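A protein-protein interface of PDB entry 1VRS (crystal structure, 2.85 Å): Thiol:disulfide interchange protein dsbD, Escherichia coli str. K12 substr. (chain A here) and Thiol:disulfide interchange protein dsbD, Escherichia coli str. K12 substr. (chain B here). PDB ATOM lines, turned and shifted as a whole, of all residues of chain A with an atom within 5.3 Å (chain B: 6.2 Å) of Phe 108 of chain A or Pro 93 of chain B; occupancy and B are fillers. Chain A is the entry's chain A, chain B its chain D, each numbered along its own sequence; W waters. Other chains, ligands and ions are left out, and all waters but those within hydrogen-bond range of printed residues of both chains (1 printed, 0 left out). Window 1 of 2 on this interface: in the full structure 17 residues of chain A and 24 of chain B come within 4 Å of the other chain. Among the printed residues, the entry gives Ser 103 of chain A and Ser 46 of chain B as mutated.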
ATOM      1  N   PHE A  11     -19.650 -33.845 -23.137  1.00  0.00           N
ATOM      2  CA  PHE A  11     -19.635 -32.498 -23.732  1.00  0.00           C
ATOM      3  C   PHE A  11     -18.310 -32.176 -24.415  1.00  0.00           C
ATOM      4  O   PHE A  11     -17.231 -32.394 -23.856  1.00  0.00           O
ATOM      5  CB  PHE A  11     -19.910 -31.435 -22.675  1.00  0.00           C
ATOM      6  CG  PHE A  11     -21.177 -31.652 -21.939  1.00  0.00           C
ATOM      7  CD1 PHE A  11     -22.395 -31.563 -22.601  1.00  0.00           C
ATOM      8  CD2 PHE A  11     -21.159 -31.987 -20.591  1.00  0.00           C
ATOM      9  CE1 PHE A  11     -23.582 -31.806 -21.935  1.00  0.00           C
ATOM     10  CE2 PHE A  11     -22.340 -32.236 -19.910  1.00  0.00           C
ATOM     11  CZ  PHE A  11     -23.558 -32.146 -20.586  1.00  0.00           C
ATOM     12  N   VAL A  12     -18.396 -31.635 -25.622  1.00  0.00           N
ATOM     13  CA  VAL A  12     -17.207 -31.296 -26.390  1.00  0.00           C
ATOM     14  C   VAL A  12     -16.632 -29.950 -26.007  1.00  0.00           C
ATOM     15  O   VAL A  12     -17.283 -29.150 -25.337  1.00  0.00           O
ATOM     16  CB  VAL A  12     -17.513 -31.271 -27.884  1.00  0.00           C
ATOM     17  CG1 VAL A  12     -18.166 -32.590 -28.285  1.00  0.00           C
ATOM     18  CG2 VAL A  12     -18.399 -30.079 -28.211  1.00  0.00           C
ATOM     19  N   GLY A 102     -22.433 -19.819 -24.710  1.00  0.00           N
ATOM     20  CA  GLY A 102     -23.428 -20.831 -25.015  1.00  0.00           C
ATOM     21  C   GLY A 102     -23.537 -21.941 -23.984  1.00  0.00           C
ATOM     22  O   GLY A 102     -22.773 -22.005 -23.024  1.00  0.00           O
ATOM     23  N   SER A 103     -24.511 -22.817 -24.191  1.00  0.00           N
ATOM     24  CA  SER A 103     -24.762 -23.939 -23.301  1.00  0.00           C
ATOM     25  C   SER A 103     -25.223 -25.136 -24.095  1.00  0.00           C
ATOM     26  O   SER A 103     -25.476 -25.048 -25.299  1.00  0.00           O
ATOM     27  CB  SER A 103     -25.840 -23.598 -22.285  1.00  0.00           C
ATOM     28  OG  SER A 103     -25.387 -22.629 -21.366  1.00  0.00           O
ATOM     29  N   ALA A 104     -25.329 -26.265 -23.404  1.00  0.00           N
ATOM     30  CA  ALA A 104     -25.778 -27.504 -24.028  1.00  0.00           C
ATOM     31  C   ALA A 104     -27.100 -27.943 -23.414  1.00  0.00           C
ATOM     32  O   ALA A 104     -27.315 -27.790 -22.204  1.00  0.00           O
ATOM     33  CB  ALA A 104     -24.745 -28.581 -23.850  1.00  0.00           C
ATOM     34  N   ALA A 106     -28.273 -30.803 -22.638  1.00  0.00           N
ATOM     35  CA  ALA A 106     -28.139 -31.783 -21.577  1.00  0.00           C
ATOM     36  C   ALA A 106     -27.805 -31.155 -20.232  1.00  0.00           C
ATOM     37  O   ALA A 106     -27.630 -31.869 -19.244  1.00  0.00           O
ATOM     38  CB  ALA A 106     -27.079 -32.802 -21.953  1.00  0.00           C
ATOM     39  N   GLY A 107     -27.699 -29.828 -20.193  1.00  0.00           N
ATOM     40  CA  GLY A 107     -27.407 -29.143 -18.943  1.00  0.00           C
ATOM     41  C   GLY A 107     -25.950 -28.845 -18.669  1.00  0.00           C
ATOM     42  O   GLY A 107     -25.386 -29.309 -17.682  1.00  0.00           O
ATOM     43  N   PHE A 108     -25.340 -28.049 -19.529  1.00  0.00           N
ATOM     44  CA  PHE A 108     -23.935 -27.710 -19.368  1.00  0.00           C
ATOM     45  C   PHE A 108     -23.739 -26.284 -19.847  1.00  0.00           C
ATOM     46  O   PHE A 108     -24.129 -25.933 -20.959  1.00  0.00           O
ATOM     47  CB  PHE A 108     -23.083 -28.683 -20.192  1.00  0.00           C
ATOM     48  CG  PHE A 108     -21.617 -28.618 -19.887  1.00  0.00           C
ATOM     49  CD1 PHE A 108     -21.151 -28.847 -18.589  1.00  0.00           C
ATOM     50  CD2 PHE A 108     -20.692 -28.350 -20.903  1.00  0.00           C
ATOM     51  CE1 PHE A 108     -19.782 -28.815 -18.297  1.00  0.00           C
ATOM     52  CE2 PHE A 108     -19.319 -28.313 -20.628  1.00  0.00           C
ATOM     53  CZ  PHE A 108     -18.865 -28.550 -19.309  1.00  0.00           C
ATOM     54  N   CYS A 109     -23.136 -25.456 -19.011  1.00  0.00           N
ATOM     55  CA  CYS A 109     -22.928 -24.069 -19.388  1.00  0.00           C
ATOM     56  C   CYS A 109     -21.472 -23.750 -19.670  1.00  0.00           C
ATOM     57  O   CYS A 109     -20.603 -23.972 -18.822  1.00  0.00           O
ATOM     58  CB  CYS A 109     -23.418 -23.139 -18.279  1.00  0.00           C
ATOM     59  SG  CYS A 109     -24.993 -23.599 -17.484  1.00  0.00           S
ATOM     60  N   TYR A 110     -21.193 -23.237 -20.860  1.00  0.00           N
ATOM     61  CA  TYR A 110     -19.833 -22.854 -21.153  1.00  0.00           C
ATOM     62  C   TYR A 110     -19.675 -21.412 -20.702  1.00  0.00           C
ATOM     63  O   TYR A 110     -20.643 -20.640 -20.681  1.00  0.00           O
ATOM     64  CB  TYR A 110     -19.540 -22.959 -22.629  1.00  0.00           C
ATOM     65  CG  TYR A 110     -19.534 -24.366 -23.136  1.00  0.00           C
ATOM     66  CD1 TYR A 110     -20.732 -25.011 -23.480  1.00  0.00           C
ATOM     67  CD2 TYR A 110     -18.330 -25.059 -23.301  1.00  0.00           C
ATOM     68  CE1 TYR A 110     -20.735 -26.316 -23.985  1.00  0.00           C
ATOM     69  CE2 TYR A 110     -18.312 -26.363 -23.806  1.00  0.00           C
ATOM     70  CZ  TYR A 110     -19.517 -26.985 -24.149  1.00  0.00           C
ATOM     71  OH  TYR A 110     -19.506 -28.256 -24.692  1.00  0.00           O
ATOM     72  N   ASP B  37     -17.215 -29.000  -5.958  1.00  0.00           N
ATOM     73  CA  ASP B  37     -18.320 -28.618  -6.816  1.00  0.00           C
ATOM     74  C   ASP B  37     -18.113 -27.217  -7.400  1.00  0.00           C
ATOM     75  O   ASP B  37     -18.071 -26.229  -6.668  1.00  0.00           O
ATOM     76  CB  ASP B  37     -19.615 -28.658  -6.024  1.00  0.00           C
ATOM     77  CG  ASP B  37     -20.755 -28.015  -6.762  1.00  0.00           C
ATOM     78  OD1 ASP B  37     -21.253 -28.618  -7.740  1.00  0.00           O
ATOM     79  OD2 ASP B  37     -21.132 -26.897  -6.362  1.00  0.00           O
ATOM     80  N   LEU B  38     -17.975 -27.145  -8.720  1.00  0.00           N
ATOM     81  CA  LEU B  38     -17.804 -25.873  -9.402  1.00  0.00           C
ATOM     82  C   LEU B  38     -19.199 -25.390  -9.809  1.00  0.00           C
ATOM     83  O   LEU B  38     -19.932 -26.067 -10.539  1.00  0.00           O
ATOM     84  CB  LEU B  38     -16.888 -26.067 -10.597  1.00  0.00           C
ATOM     85  CG  LEU B  38     -15.560 -26.653 -10.121  1.00  0.00           C
ATOM     86  CD1 LEU B  38     -15.242 -27.902 -10.930  1.00  0.00           C
ATOM     87  CD2 LEU B  38     -14.462 -25.606 -10.227  1.00  0.00           C
ATOM     88  N   TYR B  39     -19.542 -24.203  -9.323  1.00  0.00           N
ATOM     89  CA  TYR B  39     -20.855 -23.605  -9.507  1.00  0.00           C
ATOM     90  C   TYR B  39     -20.844 -22.182 -10.067  1.00  0.00           C
ATOM     91  O   TYR B  39     -19.852 -21.472  -9.941  1.00  0.00           O
ATOM     92  CB  TYR B  39     -21.520 -23.627  -8.124  1.00  0.00           C
ATOM     93  CG  TYR B  39     -22.753 -22.778  -7.957  1.00  0.00           C
ATOM     94  CD1 TYR B  39     -22.665 -21.414  -7.663  1.00  0.00           C
ATOM     95  CD2 TYR B  39     -24.017 -23.340  -8.116  1.00  0.00           C
ATOM     96  CE1 TYR B  39     -23.812 -20.634  -7.540  1.00  0.00           C
ATOM     97  CE2 TYR B  39     -25.169 -22.576  -7.994  1.00  0.00           C
ATOM     98  CZ  TYR B  39     -25.067 -21.228  -7.713  1.00  0.00           C
ATOM     99  OH  TYR B  39     -26.236 -20.496  -7.638  1.00  0.00           O
ATOM    100  N   CYS B  43     -25.493 -20.178 -14.533  1.00  0.00           N
ATOM    101  CA  CYS B  43     -25.683 -21.529 -15.057  1.00  0.00           C
ATOM    102  C   CYS B  43     -26.920 -22.245 -14.505  1.00  0.00           C
ATOM    103  O   CYS B  43     -26.956 -22.630 -13.338  1.00  0.00           O
ATOM    104  CB  CYS B  43     -24.453 -22.367 -14.755  1.00  0.00           C
ATOM    105  SG  CYS B  43     -24.462 -23.996 -15.555  1.00  0.00           S
ATOM    106  N   ALA B  45     -28.100 -25.256 -15.172  1.00  0.00           N
ATOM    107  CA  ALA B  45     -27.780 -26.629 -14.804  1.00  0.00           C
ATOM    108  C   ALA B  45     -27.142 -26.655 -13.412  1.00  0.00           C
ATOM    109  O   ALA B  45     -27.364 -27.573 -12.623  1.00  0.00           O
ATOM    110  CB  ALA B  45     -26.828 -27.231 -15.829  1.00  0.00           C
ATOM    111  N   SER B  46     -26.344 -25.635 -13.127  1.00  0.00           N
ATOM    112  CA  SER B  46     -25.676 -25.522 -11.847  1.00  0.00           C
ATOM    113  C   SER B  46     -26.739 -25.289 -10.772  1.00  0.00           C
ATOM    114  O   SER B  46     -26.612 -25.761  -9.646  1.00  0.00           O
ATOM    115  CB  SER B  46     -24.687 -24.357 -11.890  1.00  0.00           C
ATOM    116  OG  SER B  46     -23.458 -24.708 -11.287  1.00  0.00           O
ATOM    117  N   PHE B  49     -28.663 -28.486 -10.136  1.00  0.00           N
ATOM    118  CA  PHE B  49     -27.879 -29.425  -9.353  1.00  0.00           C
ATOM    119  C   PHE B  49     -28.100 -29.160  -7.882  1.00  0.00           C
ATOM    120  O   PHE B  49     -28.303 -30.087  -7.105  1.00  0.00           O
ATOM    121  CB  PHE B  49     -26.387 -29.295  -9.683  1.00  0.00           C
ATOM    122  CG  PHE B  49     -25.670 -30.621  -9.765  1.00  0.00           C
ATOM    123  CD1 PHE B  49     -25.342 -31.327  -8.609  1.00  0.00           C
ATOM    124  CD2 PHE B  49     -25.366 -31.186 -11.012  1.00  0.00           C
ATOM    125  CE1 PHE B  49     -24.726 -32.580  -8.697  1.00  0.00           C
ATOM    126  CE2 PHE B  49     -24.754 -32.431 -11.104  1.00  0.00           C
ATOM    127  CZ  PHE B  49     -24.433 -33.130  -9.947  1.00  0.00           C
ATOM    128  N   VAL B  89     -11.257 -27.571 -16.298  1.00  0.00           N
ATOM    129  CA  VAL B  89     -12.717 -27.595 -16.281  1.00  0.00           C
ATOM    130  C   VAL B  89     -13.216 -26.875 -17.536  1.00  0.00           C
ATOM    131  O   VAL B  89     -12.825 -25.743 -17.817  1.00  0.00           O
ATOM    132  CB  VAL B  89     -13.265 -26.866 -15.034  1.00  0.00           C
ATOM    133  CG1 VAL B  89     -14.784 -26.974 -14.979  1.00  0.00           C
ATOM    134  CG2 VAL B  89     -12.639 -27.447 -13.789  1.00  0.00           C
ATOM    135  N   LEU B  90     -14.076 -27.539 -18.290  1.00  0.00           N
ATOM    136  CA  LEU B  90     -14.612 -26.974 -19.520  1.00  0.00           C
ATOM    137  C   LEU B  90     -15.869 -26.126 -19.348  1.00  0.00           C
ATOM    138  O   LEU B  90     -16.119 -25.219 -20.131  1.00  0.00           O
ATOM    139  CB  LEU B  90     -14.930 -28.103 -20.491  1.00  0.00           C
ATOM    140  CG  LEU B  90     -13.916 -28.495 -21.564  1.00  0.00           C
ATOM    141  CD1 LEU B  90     -12.500 -28.591 -20.988  1.00  0.00           C
ATOM    142  CD2 LEU B  90     -14.390 -29.823 -22.197  1.00  0.00           C
ATOM    143  N   GLY B  91     -16.671 -26.438 -18.339  1.00  0.00           N
ATOM    144  CA  GLY B  91     -17.897 -25.698 -18.135  1.00  0.00           C
ATOM    145  C   GLY B  91     -18.571 -26.161 -16.867  1.00  0.00           C
ATOM    146  O   GLY B  91     -18.005 -26.971 -16.149  1.00  0.00           O
ATOM    147  N   LEU B  92     -19.775 -25.665 -16.596  1.00  0.00           N
ATOM    148  CA  LEU B  92     -20.483 -26.026 -15.377  1.00  0.00           C
ATOM    149  C   LEU B  92     -21.855 -26.560 -15.714  1.00  0.00           C
ATOM    150  O   LEU B  92     -22.395 -26.247 -16.773  1.00  0.00           O
ATOM    151  CB  LEU B  92     -20.605 -24.797 -14.492  1.00  0.00           C
ATOM    152  CG  LEU B  92     -19.330 -23.944 -14.488  1.00  0.00           C
ATOM    153  CD1 LEU B  92     -19.672 -22.548 -14.065  1.00  0.00           C
ATOM    154  CD2 LEU B  92     -18.278 -24.535 -13.576  1.00  0.00           C
ATOM    155  N   PRO B  93     -22.420 -27.416 -14.840  1.00  0.00           N
ATOM    156  CA  PRO B  93     -21.771 -27.845 -13.601  1.00  0.00           C
ATOM    157  C   PRO B  93     -20.725 -28.932 -13.818  1.00  0.00           C
ATOM    158  O   PRO B  93     -20.853 -29.783 -14.702  1.00  0.00           O
ATOM    159  CB  PRO B  93     -22.942 -28.339 -12.753  1.00  0.00           C
ATOM    160  CG  PRO B  93     -23.811 -28.970 -13.752  1.00  0.00           C
ATOM    161  CD  PRO B  93     -23.777 -27.990 -14.930  1.00  0.00           C
ATOM    162  N   THR B  94     -19.677 -28.878 -13.011  1.00  0.00           N
ATOM    163  CA  THR B  94     -18.612 -29.874 -13.068  1.00  0.00           C
ATOM    164  C   THR B  94     -18.261 -30.226 -11.641  1.00  0.00           C
ATOM    165  O   THR B  94     -18.024 -29.339 -10.815  1.00  0.00           O
ATOM    166  CB  THR B  94     -17.306 -29.350 -13.747  1.00  0.00           C
ATOM    167  OG1 THR B  94     -17.539 -29.095 -15.135  1.00  0.00           O
ATOM    168  CG2 THR B  94     -16.193 -30.390 -13.619  1.00  0.00           C
ATOM    169  N   ILE B  95     -18.216 -31.515 -11.353  1.00  0.00           N
ATOM    170  CA  ILE B  95     -17.876 -31.952 -10.012  1.00  0.00           C
ATOM    171  C   ILE B  95     -16.694 -32.932  -9.998  1.00  0.00           C
ATOM    172  O   ILE B  95     -16.693 -33.931 -10.714  1.00  0.00           O
ATOM    173  CB  ILE B  95     -19.111 -32.556  -9.348  1.00  0.00           C
ATOM    174  CG1 ILE B  95     -20.195 -31.485  -9.308  1.00  0.00           C
ATOM    175  CG2 ILE B  95     -18.781 -33.028  -7.944  1.00  0.00           C
ATOM    176  CD1 ILE B  95     -21.550 -32.002  -8.980  1.00  0.00           C
ATOM    177  N   VAL B 110     -18.114 -35.475 -12.646  1.00  0.00           N
ATOM    178  CA  VAL B 110     -19.434 -35.334 -13.231  1.00  0.00           C
ATOM    179  C   VAL B 110     -19.534 -34.008 -13.973  1.00  0.00           C
ATOM    180  O   VAL B 110     -19.258 -32.941 -13.419  1.00  0.00           O
ATOM    181  CB  VAL B 110     -20.534 -35.422 -12.139  1.00  0.00           C
ATOM    182  CG1 VAL B 110     -21.888 -34.968 -12.704  1.00  0.00           C
ATOM    183  CG2 VAL B 110     -20.619 -36.861 -11.631  1.00  0.00           C
ATOM    184  N   THR B 111     -19.901 -34.086 -15.242  1.00  0.00           N
ATOM    185  CA  THR B 111     -20.032 -32.892 -16.050  1.00  0.00           C
ATOM    186  C   THR B 111     -21.463 -32.750 -16.530  1.00  0.00           C
ATOM    187  O   THR B 111     -22.004 -33.635 -17.201  1.00  0.00           O
ATOM    188  CB  THR B 111     -19.113 -32.941 -17.258  1.00  0.00           C
ATOM    189  OG1 THR B 111     -19.301 -34.184 -17.944  1.00  0.00           O
ATOM    190  CG2 THR B 111     -17.668 -32.794 -16.822  1.00  0.00           C
ATOM    191  N   GLY B 112     -22.076 -31.628 -16.178  1.00  0.00           N
ATOM    192  CA  GLY B 112     -23.448 -31.394 -16.580  1.00  0.00           C
ATOM    193  C   GLY B 112     -24.378 -31.823 -15.468  1.00  0.00           C
ATOM    194  O   GLY B 112     -23.935 -32.397 -14.481  1.00  0.00           O
ATOM    195  N   PHE B 113     -25.664 -31.543 -15.610  1.00  0.00           N
ATOM    196  CA  PHE B 113     -26.601 -31.924 -14.570  1.00  0.00           C
ATOM    197  C   PHE B 113     -26.765 -33.430 -14.497  1.00  0.00           C
ATOM    198  O   PHE B 113     -26.706 -34.127 -15.507  1.00  0.00           O
ATOM    199  CB  PHE B 113     -27.972 -31.309 -14.813  1.00  0.00           C
ATOM    200  CG  PHE B 113     -29.002 -31.736 -13.809  1.00  0.00           C
ATOM    201  CD1 PHE B 113     -29.145 -31.055 -12.609  1.00  0.00           C
ATOM    202  CD2 PHE B 113     -29.800 -32.845 -14.047  1.00  0.00           C
ATOM    203  CE1 PHE B 113     -30.078 -31.478 -11.650  1.00  0.00           C
ATOM    204  CE2 PHE B 113     -30.728 -33.274 -13.106  1.00  0.00           C
ATOM    205  CZ  PHE B 113     -30.868 -32.591 -11.904  1.00  0.00           C
ATOM    206  N   MET B 114     -26.984 -33.918 -13.284  1.00  0.00           N
ATOM    207  CA  MET B 114     -27.183 -35.339 -13.042  1.00  0.00           C
ATOM    208  C   MET B 114     -28.225 -35.423 -11.932  1.00  0.00           C
ATOM    209  O   MET B 114     -28.156 -34.678 -10.954  1.00  0.00           O
ATOM    210  CB  MET B 114     -25.867 -35.988 -12.595  1.00  0.00           C
ATOM    211  CG  MET B 114     -25.882 -37.517 -12.561  1.00  0.00           C
ATOM    212  SD  MET B 114     -24.347 -38.261 -11.911  1.00  0.00           S
ATOM    213  CE  MET B 114     -23.448 -38.551 -13.420  1.00  0.00           C
HETATM  214  O   HOH W   1     -25.788 -33.988 -18.372  1.00  0.00           O
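The side-chain sulfur of Cys 43 of chain B lies within hydrogen-bond range of the backbone NH of Ser 46 of chain B, at 3.5 Å.
O of Val 12 of chain A sits at hydrogen-bond distance from OH of Tyr 110 of chain A (2.5 Å).
N of Tyr 110 of chain A lies within hydrogen-bond range of O of Gly 102 of chain A (2.9 Å).
The backbone carbonyl oxygen (O) of Pro 93 of chain B lies within hydrogen-bond range of the backbone NH (N) of Gly 112 of chain B (2.7 Å).
The backbone carbonyl oxygen of Thr 94 of chain B is in hydrogen-bond range of the backbone NH of Leu 38 of chain B (3.0 Å).
Gly 112 of chain B touches Phe 11 of chain A.
Gly 107 of chain A touches Ala 45 of chain B (O to CB, 3.1 Å).
O of Gly 107 of chain A touches CD of Pro 93 of chain B, 3.4 Å away.
Gly 112 of chain B touches Gly 107 of chain A.
Phe 108 of chain A touches Leu 90 of chain B.
N of Gly 91 of chain B touches CZ of Phe 108 of chain A, 3.2 Å away.
Phe 108 of chain A touches Pro 93 of chain B (CE1 to O, 3.9 Å).
Thr 94 of chain B touches Phe 108 of chain A (OG1 to CE1, 3.9 Å).
CD1 of Phe 108 of chain A touches N of Gly 112 of chain B (3.8 Å).
Tyr 110 of chain A touches Leu 90 of chain B.
Of the 10 printed residues of chain A, 5 touch a printed residue of chain B.
Printed residues of chain A that touch a printed residue of chain B: Phe 11, Gly 107, Phe 108, Cys 109 and Tyr 110.
Hydrophobic or aromatic side chains of chain B that line the printed part of chain A: Ala 45 and Pro 93.
Among the printed residues, no Asp or Glu carboxylate lies within 4 Å of a Lys or Arg side-chain nitrogen of the other chain.
The backbone carbonyl oxygen of Leu 92 of chain B lies within hydrogen-bond range of the backbone NH of Cys 109 of chain A (2.5 Å).
N of Phe 113 of chain B is in hydrogen-bond range of O of Gly 107 of chain A (3.1 Å).
The side-chain sulfur (SG) of Cys 43 of chain B forms a disulfide with the side-chain sulfur (SG) of Cys 109 of chain A.
Ala 104 of chain A touches none of the printed residues of chain B.
Of chain B, only Leu 90 (3.9 Å), Gly 91 (3.2 Å), Leu 92 (3.4 Å), Pro 93 (3.9 Å), Thr 94 (3.9 Å) and Gly 112 (3.8 Å) come within 4 Å of Phe 108 of chain A.
Printed residues of chain A within 4 Å of Ala 45 of chain B: Gly 107 (3.1 Å).
Printed residues of chain A within 4 Å of Gly 91 of chain B: Phe 108 and Cys 109.
Of the printed residues of chain A, Leu 92 of chain B touches Phe 108 and Cys 109.
Pro 93 of chain B touches two residues of chain A.
Of the printed residues of chain A, Thr 94 of chain B touches Phe 108.
The nearest residue of chain B that does not touch Phe 108 of chain A is Ala 45 of chain B (4.1 Å).
The nearest printed residue of chain A that does not touch Phe 113 of chain B is Ala 106 of chain A (4.1 Å).
Water W1 bridges O of Ala 106 of chain A (2.9 Å) and O of Phe 113 of chain B (3.0 Å).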
